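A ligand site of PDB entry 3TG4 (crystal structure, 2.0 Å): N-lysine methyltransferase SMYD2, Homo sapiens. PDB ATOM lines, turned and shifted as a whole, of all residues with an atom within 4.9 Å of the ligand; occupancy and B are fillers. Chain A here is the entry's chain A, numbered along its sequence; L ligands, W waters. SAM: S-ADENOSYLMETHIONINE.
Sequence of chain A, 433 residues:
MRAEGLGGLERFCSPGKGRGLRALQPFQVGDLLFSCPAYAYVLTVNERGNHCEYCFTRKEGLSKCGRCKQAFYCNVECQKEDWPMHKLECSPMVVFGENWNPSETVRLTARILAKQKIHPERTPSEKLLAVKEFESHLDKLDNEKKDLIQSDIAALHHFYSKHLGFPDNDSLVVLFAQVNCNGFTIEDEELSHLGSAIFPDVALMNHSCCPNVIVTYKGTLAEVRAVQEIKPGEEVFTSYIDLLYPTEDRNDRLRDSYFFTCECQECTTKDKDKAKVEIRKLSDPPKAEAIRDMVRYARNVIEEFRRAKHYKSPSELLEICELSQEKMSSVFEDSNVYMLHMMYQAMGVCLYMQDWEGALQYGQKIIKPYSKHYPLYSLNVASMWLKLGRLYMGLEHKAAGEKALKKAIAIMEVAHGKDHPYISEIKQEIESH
O3' of the ligand is in hydrogen-bond range of O of Tyr 258. OXT of the ligand sits at hydrogen-bond distance from N of Arg 19 (2.7 Å). O of Arg 19 lies within hydrogen-bond range of N of the ligand, 2.9 Å away. The guanidinium group (NH2) of Arg 19 lies within salt-bridge range of an oxygen (O) of the ligand, at 2.7 Å. An oxygen (O3') of the ligand sits at hydrogen-bond distance from a ring nitrogen (NE2) of His 137 (2.8 Å). The backbone carbonyl oxygen (O) of Lys 17 sits at hydrogen-bond distance from a nitrogen (N) of the ligand, at 2.8 Å. ND2 of Asn 206 lies close to N of the ligand (2.9 Å). The backbone NH (N) of His 207 is in hydrogen-bond range of a nitrogen (N7) of the ligand. The backbone carbonyl oxygen (O) of His 207 lies within hydrogen-bond range of a nitrogen (N6) of the ligand (3.0 Å). An oxygen (O3') of the ligand lies within hydrogen-bond range of the side-chain sulfur (SG) of Cys 181 (3.6 Å).
NE2 of His 137 lies within hydrogen-bond range of O of Tyr 258 (3.4 Å). O of Arg 19 lies close to OD1 of Asn 206. The backbone NH of His 137 lies within hydrogen-bond range of the side-chain carboxylate of Glu 135 (3.1 Å). The backbone carbonyl oxygen of Met 205 lies within hydrogen-bond range of the side-chain hydroxyl of Tyr 240, at 2.7 Å. SG of Cys 181 sits close to OD1 of Asn 182, 3.8 Å away. The side-chain amide oxygen (OD1) of Asn 182 lies close to the backbone carbonyl oxygen (O) of Glu 135 (3.0 Å). The backbone carbonyl oxygen (O) of Glu 135 sits close to the side-chain sulfur (SG) of Cys 181 (3.6 Å).
A sulfur (SD) of the ligand lies close to the side-chain amide nitrogen (ND2) of Asn 182, at 3.5 Å. SD of the ligand sits close to O of Ala 203 (3.6 Å). The side-chain hydroxyl of Tyr 240 sits close to a sulfur (SD) of the ligand, 3.8 Å away. Gly 16 touches the ligand (O to C2, 3.3 Å). C of Gly 18 touches OXT of the ligand, at 3.8 Å. O of Leu 204 touches CB of the ligand (3.5 Å). Met 205 touches the ligand. CD1 of Phe 260 touches N1 of the ligand, 3.4 Å away. Hydrophobic or aromatic side chains within 4 Å of the ligand: His 137, His 207, Tyr 240, Tyr 258 and Phe 260. Within 4 Å of the ligand: Gly 16, Lys 17, Gly 18, Arg 19, His 137, Cys 181, Asn 182, Ala 203, Leu 204, Met 205, Asn 206, His 207, Tyr 240, Tyr 258 and Phe 260.
Water W1 lies within hydrogen-bond range of N of Glu 135, O of the ligand and ND2 of Asn 182. Water W6 lies within hydrogen-bond range of an oxygen (OXT) of the ligand (2.9 Å) and the side-chain carboxylate of Glu 135 (3.2 Å). Water W3 lies within hydrogen-bond range of the backbone carbonyl oxygen of His 207 (2.7 Å) and a nitrogen (N6) of the ligand (3.3 Å).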
ATOM      1  N   GLY A  16       9.529   1.716 -13.736  1.00  0.00           N
ATOM      2  CA  GLY A  16       9.381   0.820 -14.882  1.00  0.00           C
ATOM      3  C   GLY A  16       8.009   0.194 -15.083  1.00  0.00           C
ATOM      4  O   GLY A  16       7.861  -0.692 -15.920  1.00  0.00           O
ATOM      5  N   LYS A  17       7.014   0.630 -14.311  1.00  0.00           N
ATOM      6  CA  LYS A  17       5.672   0.008 -14.344  1.00  0.00           C
ATOM      7  C   LYS A  17       4.551   1.027 -14.419  1.00  0.00           C
ATOM      8  O   LYS A  17       3.386   0.683 -14.262  1.00  0.00           O
ATOM      9  CB  LYS A  17       5.440  -0.918 -13.132  1.00  0.00           C
ATOM     10  CG  LYS A  17       6.427  -2.068 -12.988  1.00  0.00           C
ATOM     11  CD  LYS A  17       6.168  -2.892 -11.729  1.00  0.00           C
ATOM     12  CE  LYS A  17       7.068  -4.104 -11.644  1.00  0.00           C
ATOM     13  NZ  LYS A  17       8.474  -3.764 -11.206  1.00  0.00           N
ATOM     14  N   GLY A  18       4.903   2.295 -14.659  1.00  0.00           N
ATOM     15  CA  GLY A  18       3.892   3.368 -14.623  1.00  0.00           C
ATOM     16  C   GLY A  18       3.378   3.539 -13.195  1.00  0.00           C
ATOM     17  O   GLY A  18       4.171   3.504 -12.249  1.00  0.00           O
ATOM     18  N   ARG A  19       2.078   3.726 -13.054  1.00  0.00           N
ATOM     19  CA  ARG A  19       1.427   3.884 -11.750  1.00  0.00           C
ATOM     20  C   ARG A  19       1.049   2.542 -11.131  1.00  0.00           C
ATOM     21  O   ARG A  19       0.746   1.580 -11.848  1.00  0.00           O
ATOM     22  CB  ARG A  19       0.174   4.763 -11.853  1.00  0.00           C
ATOM     23  CG  ARG A  19       0.459   6.220 -12.339  1.00  0.00           C
ATOM     24  CD  ARG A  19      -0.797   6.855 -12.964  1.00  0.00           C
ATOM     25  NE  ARG A  19      -1.369   6.037 -14.026  1.00  0.00           N
ATOM     26  CZ  ARG A  19      -2.346   6.424 -14.856  1.00  0.00           C
ATOM     27  NH1 ARG A  19      -2.859   7.645 -14.769  1.00  0.00           N
ATOM     28  NH2 ARG A  19      -2.792   5.585 -15.785  1.00  0.00           N
ATOM     29  N   LEU A 129      -7.923   6.024  -9.206  1.00  0.00           N
ATOM     30  CA  LEU A 129      -7.669   6.058 -10.641  1.00  0.00           C
ATOM     31  C   LEU A 129      -8.979   6.224 -11.394  1.00  0.00           C
ATOM     32  O   LEU A 129      -9.934   5.470 -11.172  1.00  0.00           O
ATOM     33  CB  LEU A 129      -6.965   4.768 -11.100  1.00  0.00           C
ATOM     34  CG  LEU A 129      -6.689   4.591 -12.593  1.00  0.00           C
ATOM     35  CD1 LEU A 129      -5.764   5.687 -13.125  1.00  0.00           C
ATOM     36  CD2 LEU A 129      -6.103   3.217 -12.875  1.00  0.00           C
ATOM     37  N   GLU A 135      -4.271   4.081 -18.816  1.00  0.00           N
ATOM     38  CA  GLU A 135      -3.264   3.906 -19.860  1.00  0.00           C
ATOM     39  C   GLU A 135      -3.902   3.285 -21.095  1.00  0.00           C
ATOM     40  O   GLU A 135      -4.728   2.380 -20.973  1.00  0.00           O
ATOM     41  CB  GLU A 135      -2.108   3.020 -19.356  1.00  0.00           C
ATOM     42  CG  GLU A 135      -0.964   2.862 -20.364  1.00  0.00           C
ATOM     43  CD  GLU A 135      -0.375   4.204 -20.785  1.00  0.00           C
ATOM     44  OE1 GLU A 135       0.331   4.813 -19.959  1.00  0.00           O
ATOM     45  OE2 GLU A 135      -0.635   4.653 -21.929  1.00  0.00           O
ATOM     46  N   HIS A 137      -1.715   2.832 -24.159  1.00  0.00           N
ATOM     47  CA  HIS A 137      -0.609   2.361 -25.021  1.00  0.00           C
ATOM     48  C   HIS A 137      -0.887   2.668 -26.518  1.00  0.00           C
ATOM     49  O   HIS A 137      -0.530   1.901 -27.418  1.00  0.00           O
ATOM     50  CB  HIS A 137      -0.323   0.870 -24.820  1.00  0.00           C
ATOM     51  CG  HIS A 137       0.226   0.526 -23.466  1.00  0.00           C
ATOM     52  ND1 HIS A 137       1.374   1.096 -22.962  1.00  0.00           N
ATOM     53  CD2 HIS A 137      -0.189  -0.362 -22.532  1.00  0.00           C
ATOM     54  CE1 HIS A 137       1.628   0.599 -21.767  1.00  0.00           C
ATOM     55  NE2 HIS A 137       0.700  -0.291 -21.477  1.00  0.00           N
ATOM     56  N   CYS A 181      -6.531  -2.342 -22.312  1.00  0.00           N
ATOM     57  CA  CYS A 181      -5.467  -2.349 -21.286  1.00  0.00           C
ATOM     58  C   CYS A 181      -5.995  -2.605 -19.864  1.00  0.00           C
ATOM     59  O   CYS A 181      -5.296  -3.209 -19.031  1.00  0.00           O
ATOM     60  CB  CYS A 181      -4.640  -1.036 -21.356  1.00  0.00           C
ATOM     61  SG  CYS A 181      -3.315  -0.869 -20.124  1.00  0.00           S
ATOM     62  N   ASN A 182      -7.219  -2.151 -19.594  1.00  0.00           N
ATOM     63  CA  ASN A 182      -7.732  -2.023 -18.227  1.00  0.00           C
ATOM     64  C   ASN A 182      -9.005  -2.813 -17.932  1.00  0.00           C
ATOM     65  O   ASN A 182      -9.456  -2.861 -16.780  1.00  0.00           O
ATOM     66  CB  ASN A 182      -7.978  -0.543 -17.903  1.00  0.00           C
ATOM     67  CG  ASN A 182      -6.722   0.271 -17.935  1.00  0.00           C
ATOM     68  OD1 ASN A 182      -6.423   0.945 -18.925  1.00  0.00           O
ATOM     69  ND2 ASN A 182      -5.945   0.178 -16.870  1.00  0.00           N
ATOM     70  N   ALA A 203      -7.918  -1.587 -11.541  1.00  0.00           N
ATOM     71  CA  ALA A 203      -7.067  -1.482 -12.714  1.00  0.00           C
ATOM     72  C   ALA A 203      -5.733  -0.828 -12.370  1.00  0.00           C
ATOM     73  O   ALA A 203      -4.776  -0.929 -13.132  1.00  0.00           O
ATOM     74  CB  ALA A 203      -7.764  -0.670 -13.811  1.00  0.00           C
ATOM     75  N   LEU A 204      -5.678  -0.135 -11.227  1.00  0.00           N
ATOM     76  CA  LEU A 204      -4.436   0.485 -10.778  1.00  0.00           C
ATOM     77  C   LEU A 204      -3.345  -0.549 -10.475  1.00  0.00           C
ATOM     78  O   LEU A 204      -2.158  -0.258 -10.603  1.00  0.00           O
ATOM     79  CB  LEU A 204      -4.692   1.415  -9.591  1.00  0.00           C
ATOM     80  CG  LEU A 204      -3.486   2.154  -8.951  1.00  0.00           C
ATOM     81  CD1 LEU A 204      -2.734   3.003  -9.973  1.00  0.00           C
ATOM     82  CD2 LEU A 204      -3.913   2.977  -7.750  1.00  0.00           C
ATOM     83  N   MET A 205      -3.741  -1.760 -10.095  1.00  0.00           N
ATOM     84  CA  MET A 205      -2.751  -2.749  -9.652  1.00  0.00           C
ATOM     85  C   MET A 205      -1.976  -3.344 -10.816  1.00  0.00           C
ATOM     86  O   MET A 205      -2.553  -3.790 -11.804  1.00  0.00           O
ATOM     87  CB  MET A 205      -3.427  -3.870  -8.868  1.00  0.00           C
ATOM     88  CG  MET A 205      -3.860  -3.459  -7.476  1.00  0.00           C
ATOM     89  SD  MET A 205      -4.693  -4.799  -6.620  1.00  0.00           S
ATOM     90  CE  MET A 205      -6.238  -4.943  -7.510  1.00  0.00           C
ATOM     91  N   ASN A 206      -0.655  -3.371 -10.641  1.00  0.00           N
ATOM     92  CA  ASN A 206       0.258  -3.967 -11.601  1.00  0.00           C
ATOM     93  C   ASN A 206       0.279  -5.489 -11.533  1.00  0.00           C
ATOM     94  O   ASN A 206      -0.291  -6.100 -10.627  1.00  0.00           O
ATOM     95  CB  ASN A 206       1.659  -3.356 -11.432  1.00  0.00           C
ATOM     96  CG  ASN A 206       1.701  -1.909 -11.909  1.00  0.00           C
ATOM     97  OD1 ASN A 206       2.342  -1.042 -11.312  1.00  0.00           O
ATOM     98  ND2 ASN A 206       0.975  -1.636 -12.975  1.00  0.00           N
ATOM     99  N   HIS A 207       0.929  -6.105 -12.524  1.00  0.00           N
ATOM    100  CA  HIS A 207       0.990  -7.557 -12.611  1.00  0.00           C
ATOM    101  C   HIS A 207       2.256  -8.174 -11.995  1.00  0.00           C
ATOM    102  O   HIS A 207       3.343  -7.560 -11.995  1.00  0.00           O
ATOM    103  CB  HIS A 207       0.871  -8.006 -14.071  1.00  0.00           C
ATOM    104  CG  HIS A 207       1.170  -9.468 -14.262  1.00  0.00           C
ATOM    105  ND1 HIS A 207       2.451  -9.929 -14.497  1.00  0.00           N
ATOM    106  CD2 HIS A 207       0.382 -10.561 -14.202  1.00  0.00           C
ATOM    107  CE1 HIS A 207       2.431 -11.243 -14.586  1.00  0.00           C
ATOM    108  NE2 HIS A 207       1.187 -11.658 -14.402  1.00  0.00           N
ATOM    109  N   PHE A 237       0.232  -6.574  -6.171  1.00  0.00           N
ATOM    110  CA  PHE A 237       0.164  -7.160  -7.518  1.00  0.00           C
ATOM    111  C   PHE A 237      -0.938  -8.220  -7.656  1.00  0.00           C
ATOM    112  O   PHE A 237      -1.078  -9.095  -6.799  1.00  0.00           O
ATOM    113  CB  PHE A 237       1.496  -7.841  -7.864  1.00  0.00           C
ATOM    114  CG  PHE A 237       2.683  -6.915  -7.967  1.00  0.00           C
ATOM    115  CD1 PHE A 237       2.859  -6.093  -9.079  1.00  0.00           C
ATOM    116  CD2 PHE A 237       3.665  -6.905  -6.962  1.00  0.00           C
ATOM    117  CE1 PHE A 237       3.967  -5.260  -9.187  1.00  0.00           C
ATOM    118  CE2 PHE A 237       4.794  -6.061  -7.068  1.00  0.00           C
ATOM    119  CZ  PHE A 237       4.955  -5.244  -8.176  1.00  0.00           C
ATOM    120  N   TYR A 240      -2.447 -10.878 -14.191  1.00  0.00           N
ATOM    121  CA  TYR A 240      -3.300 -10.557 -15.329  1.00  0.00           C
ATOM    122  C   TYR A 240      -3.617 -11.792 -16.163  1.00  0.00           C
ATOM    123  O   TYR A 240      -4.505 -11.762 -16.994  1.00  0.00           O
ATOM    124  CB  TYR A 240      -2.602  -9.557 -16.256  1.00  0.00           C
ATOM    125  CG  TYR A 240      -2.365  -8.150 -15.710  1.00  0.00           C
ATOM    126  CD1 TYR A 240      -2.657  -7.815 -14.382  1.00  0.00           C
ATOM    127  CD2 TYR A 240      -1.812  -7.173 -16.524  1.00  0.00           C
ATOM    128  CE1 TYR A 240      -2.431  -6.521 -13.903  1.00  0.00           C
ATOM    129  CE2 TYR A 240      -1.573  -5.878 -16.042  1.00  0.00           C
ATOM    130  CZ  TYR A 240      -1.896  -5.561 -14.735  1.00  0.00           C
ATOM    131  OH  TYR A 240      -1.655  -4.295 -14.262  1.00  0.00           O
ATOM    132  N   TYR A 258      -0.610  -6.444 -23.140  1.00  0.00           N
ATOM    133  CA  TYR A 258      -0.361  -5.390 -22.156  1.00  0.00           C
ATOM    134  C   TYR A 258       0.921  -4.590 -22.401  1.00  0.00           C
ATOM    135  O   TYR A 258       1.210  -3.641 -21.659  1.00  0.00           O
ATOM    136  CB  TYR A 258      -0.371  -5.987 -20.729  1.00  0.00           C
ATOM    137  CG  TYR A 258      -1.712  -6.574 -20.341  1.00  0.00           C
ATOM    138  CD1 TYR A 258      -2.805  -5.737 -20.071  1.00  0.00           C
ATOM    139  CD2 TYR A 258      -1.912  -7.953 -20.294  1.00  0.00           C
ATOM    140  CE1 TYR A 258      -4.053  -6.280 -19.730  1.00  0.00           C
ATOM    141  CE2 TYR A 258      -3.151  -8.496 -19.963  1.00  0.00           C
ATOM    142  CZ  TYR A 258      -4.211  -7.654 -19.680  1.00  0.00           C
ATOM    143  OH  TYR A 258      -5.432  -8.167 -19.360  1.00  0.00           O
ATOM    144  N   PHE A 259       1.673  -4.978 -23.418  1.00  0.00           N
ATOM    145  CA  PHE A 259       2.921  -4.292 -23.842  1.00  0.00           C
ATOM    146  C   PHE A 259       3.999  -4.146 -22.756  1.00  0.00           C
ATOM    147  O   PHE A 259       4.659  -3.108 -22.657  1.00  0.00           O
ATOM    148  CB  PHE A 259       2.616  -2.929 -24.476  1.00  0.00           C
ATOM    149  CG  PHE A 259       1.586  -2.982 -25.580  1.00  0.00           C
ATOM    150  CD1 PHE A 259       1.970  -3.281 -26.895  1.00  0.00           C
ATOM    151  CD2 PHE A 259       0.247  -2.708 -25.314  1.00  0.00           C
ATOM    152  CE1 PHE A 259       1.016  -3.313 -27.924  1.00  0.00           C
ATOM    153  CE2 PHE A 259      -0.705  -2.734 -26.350  1.00  0.00           C
ATOM    154  CZ  PHE A 259      -0.316  -3.045 -27.660  1.00  0.00           C
ATOM    155  N   PHE A 260       4.177  -5.177 -21.941  1.00  0.00           N
ATOM    156  CA  PHE A 260       5.333  -5.230 -21.046  1.00  0.00           C
ATOM    157  C   PHE A 260       5.864  -6.645 -20.917  1.00  0.00           C
ATOM    158  O   PHE A 260       5.149  -7.617 -21.226  1.00  0.00           O
ATOM    159  CB  PHE A 260       5.004  -4.632 -19.661  1.00  0.00           C
ATOM    160  CG  PHE A 260       4.127  -5.517 -18.804  1.00  0.00           C
ATOM    161  CD1 PHE A 260       4.700  -6.353 -17.850  1.00  0.00           C
ATOM    162  CD2 PHE A 260       2.734  -5.515 -18.953  1.00  0.00           C
ATOM    163  CE1 PHE A 260       3.903  -7.170 -17.050  1.00  0.00           C
ATOM    164  CE2 PHE A 260       1.937  -6.332 -18.153  1.00  0.00           C
ATOM    165  CZ  PHE A 260       2.533  -7.168 -17.205  1.00  0.00           C
ATOM    166  N   THR A 261       7.116  -6.741 -20.476  1.00  0.00           N
ATOM    167  CA  THR A 261       7.710  -7.989 -20.028  1.00  0.00           C
ATOM    168  C   THR A 261       7.833  -7.959 -18.497  1.00  0.00           C
ATOM    169  O   THR A 261       8.330  -6.989 -17.908  1.00  0.00           O
ATOM    170  CB  THR A 261       9.114  -8.229 -20.656  1.00  0.00           C
ATOM    171  OG1 THR A 261       9.017  -8.211 -22.090  1.00  0.00           O
ATOM    172  CG2 THR A 261       9.709  -9.564 -20.212  1.00  0.00           C
ATOM    173  N   CYS A 262       7.372  -9.031 -17.866  1.00  0.00           N
ATOM    174  CA  CYS A 262       7.400  -9.154 -16.417  1.00  0.00           C
ATOM    175  C   CYS A 262       8.773  -9.580 -15.934  1.00  0.00           C
ATOM    176  O   CYS A 262       9.433 -10.430 -16.562  1.00  0.00           O
ATOM    177  CB  CYS A 262       6.359 -10.157 -15.946  1.00  0.00           C
ATOM    178  SG  CYS A 262       6.271 -10.342 -14.158  1.00  0.00           S
HETATM  179  N   SAM L   1       0.605   0.738 -14.580  1.00  0.00           N
HETATM  180  CA  SAM L   1      -0.807   1.071 -14.938  1.00  0.00           C
HETATM  181  C   SAM L   1      -1.072   2.568 -14.881  1.00  0.00           C
HETATM  182  O   SAM L   1      -2.206   3.033 -15.127  1.00  0.00           O
HETATM  183  OXT SAM L   1      -0.168   3.371 -14.595  1.00  0.00           O
HETATM  184  CB  SAM L   1      -1.802   0.312 -14.052  1.00  0.00           C
HETATM  185  CG  SAM L   1      -2.002  -1.133 -14.514  1.00  0.00           C
HETATM  186  SD  SAM L   1      -2.818  -1.232 -16.134  1.00  0.00           S
HETATM  187  CE  SAM L   1      -4.166  -2.385 -15.744  1.00  0.00           C
HETATM  188  C5' SAM L   1      -1.795  -2.340 -17.122  1.00  0.00           C
HETATM  189  C4' SAM L   1      -0.478  -1.676 -17.559  1.00  0.00           C
HETATM  190  O4' SAM L   1       0.398  -1.446 -16.457  1.00  0.00           O
HETATM  191  C3' SAM L   1       0.312  -2.547 -18.495  1.00  0.00           C
HETATM  192  O3' SAM L   1      -0.113  -2.381 -19.817  1.00  0.00           O
HETATM  193  C2' SAM L   1       1.743  -2.070 -18.295  1.00  0.00           C
HETATM  194  O2' SAM L   1       1.986  -0.902 -19.074  1.00  0.00           O
HETATM  195  C1' SAM L   1       1.747  -1.691 -16.842  1.00  0.00           C
HETATM  196  N9  SAM L   1       2.296  -2.783 -15.994  1.00  0.00           N
HETATM  197  C8  SAM L   1       1.564  -3.567 -15.137  1.00  0.00           C
HETATM  198  N7  SAM L   1       2.396  -4.438 -14.535  1.00  0.00           N
HETATM  199  C5  SAM L   1       3.657  -4.225 -14.981  1.00  0.00           C
HETATM  200  C6  SAM L   1       4.876  -4.841 -14.690  1.00  0.00           C
HETATM  201  N6  SAM L   1       4.919  -5.842 -13.808  1.00  0.00           N
HETATM  202  N1  SAM L   1       6.025  -4.420 -15.324  1.00  0.00           N
HETATM  203  C2  SAM L   1       5.969  -3.382 -16.246  1.00  0.00           C
HETATM  204  N3  SAM L   1       4.755  -2.767 -16.523  1.00  0.00           N
HETATM  205  C4  SAM L   1       3.618  -3.181 -15.907  1.00  0.00           C
HETATM  206  O   HOH W   1      -4.426   2.463 -16.625  1.00  0.00           O
HETATM  207  O   HOH W   2       7.762  -7.088 -13.472  1.00  0.00           O
HETATM  208  O   HOH W   3       6.004  -8.119 -11.692  1.00  0.00           O
HETATM  209  O   HOH W   4       1.524   1.351 -17.236  1.00  0.00           O
HETATM  210  O   HOH W   5       4.946  -0.683 -18.347  1.00  0.00           O
HETATM  211  O   HOH W   6       0.881   4.982 -16.771  1.00  0.00           O
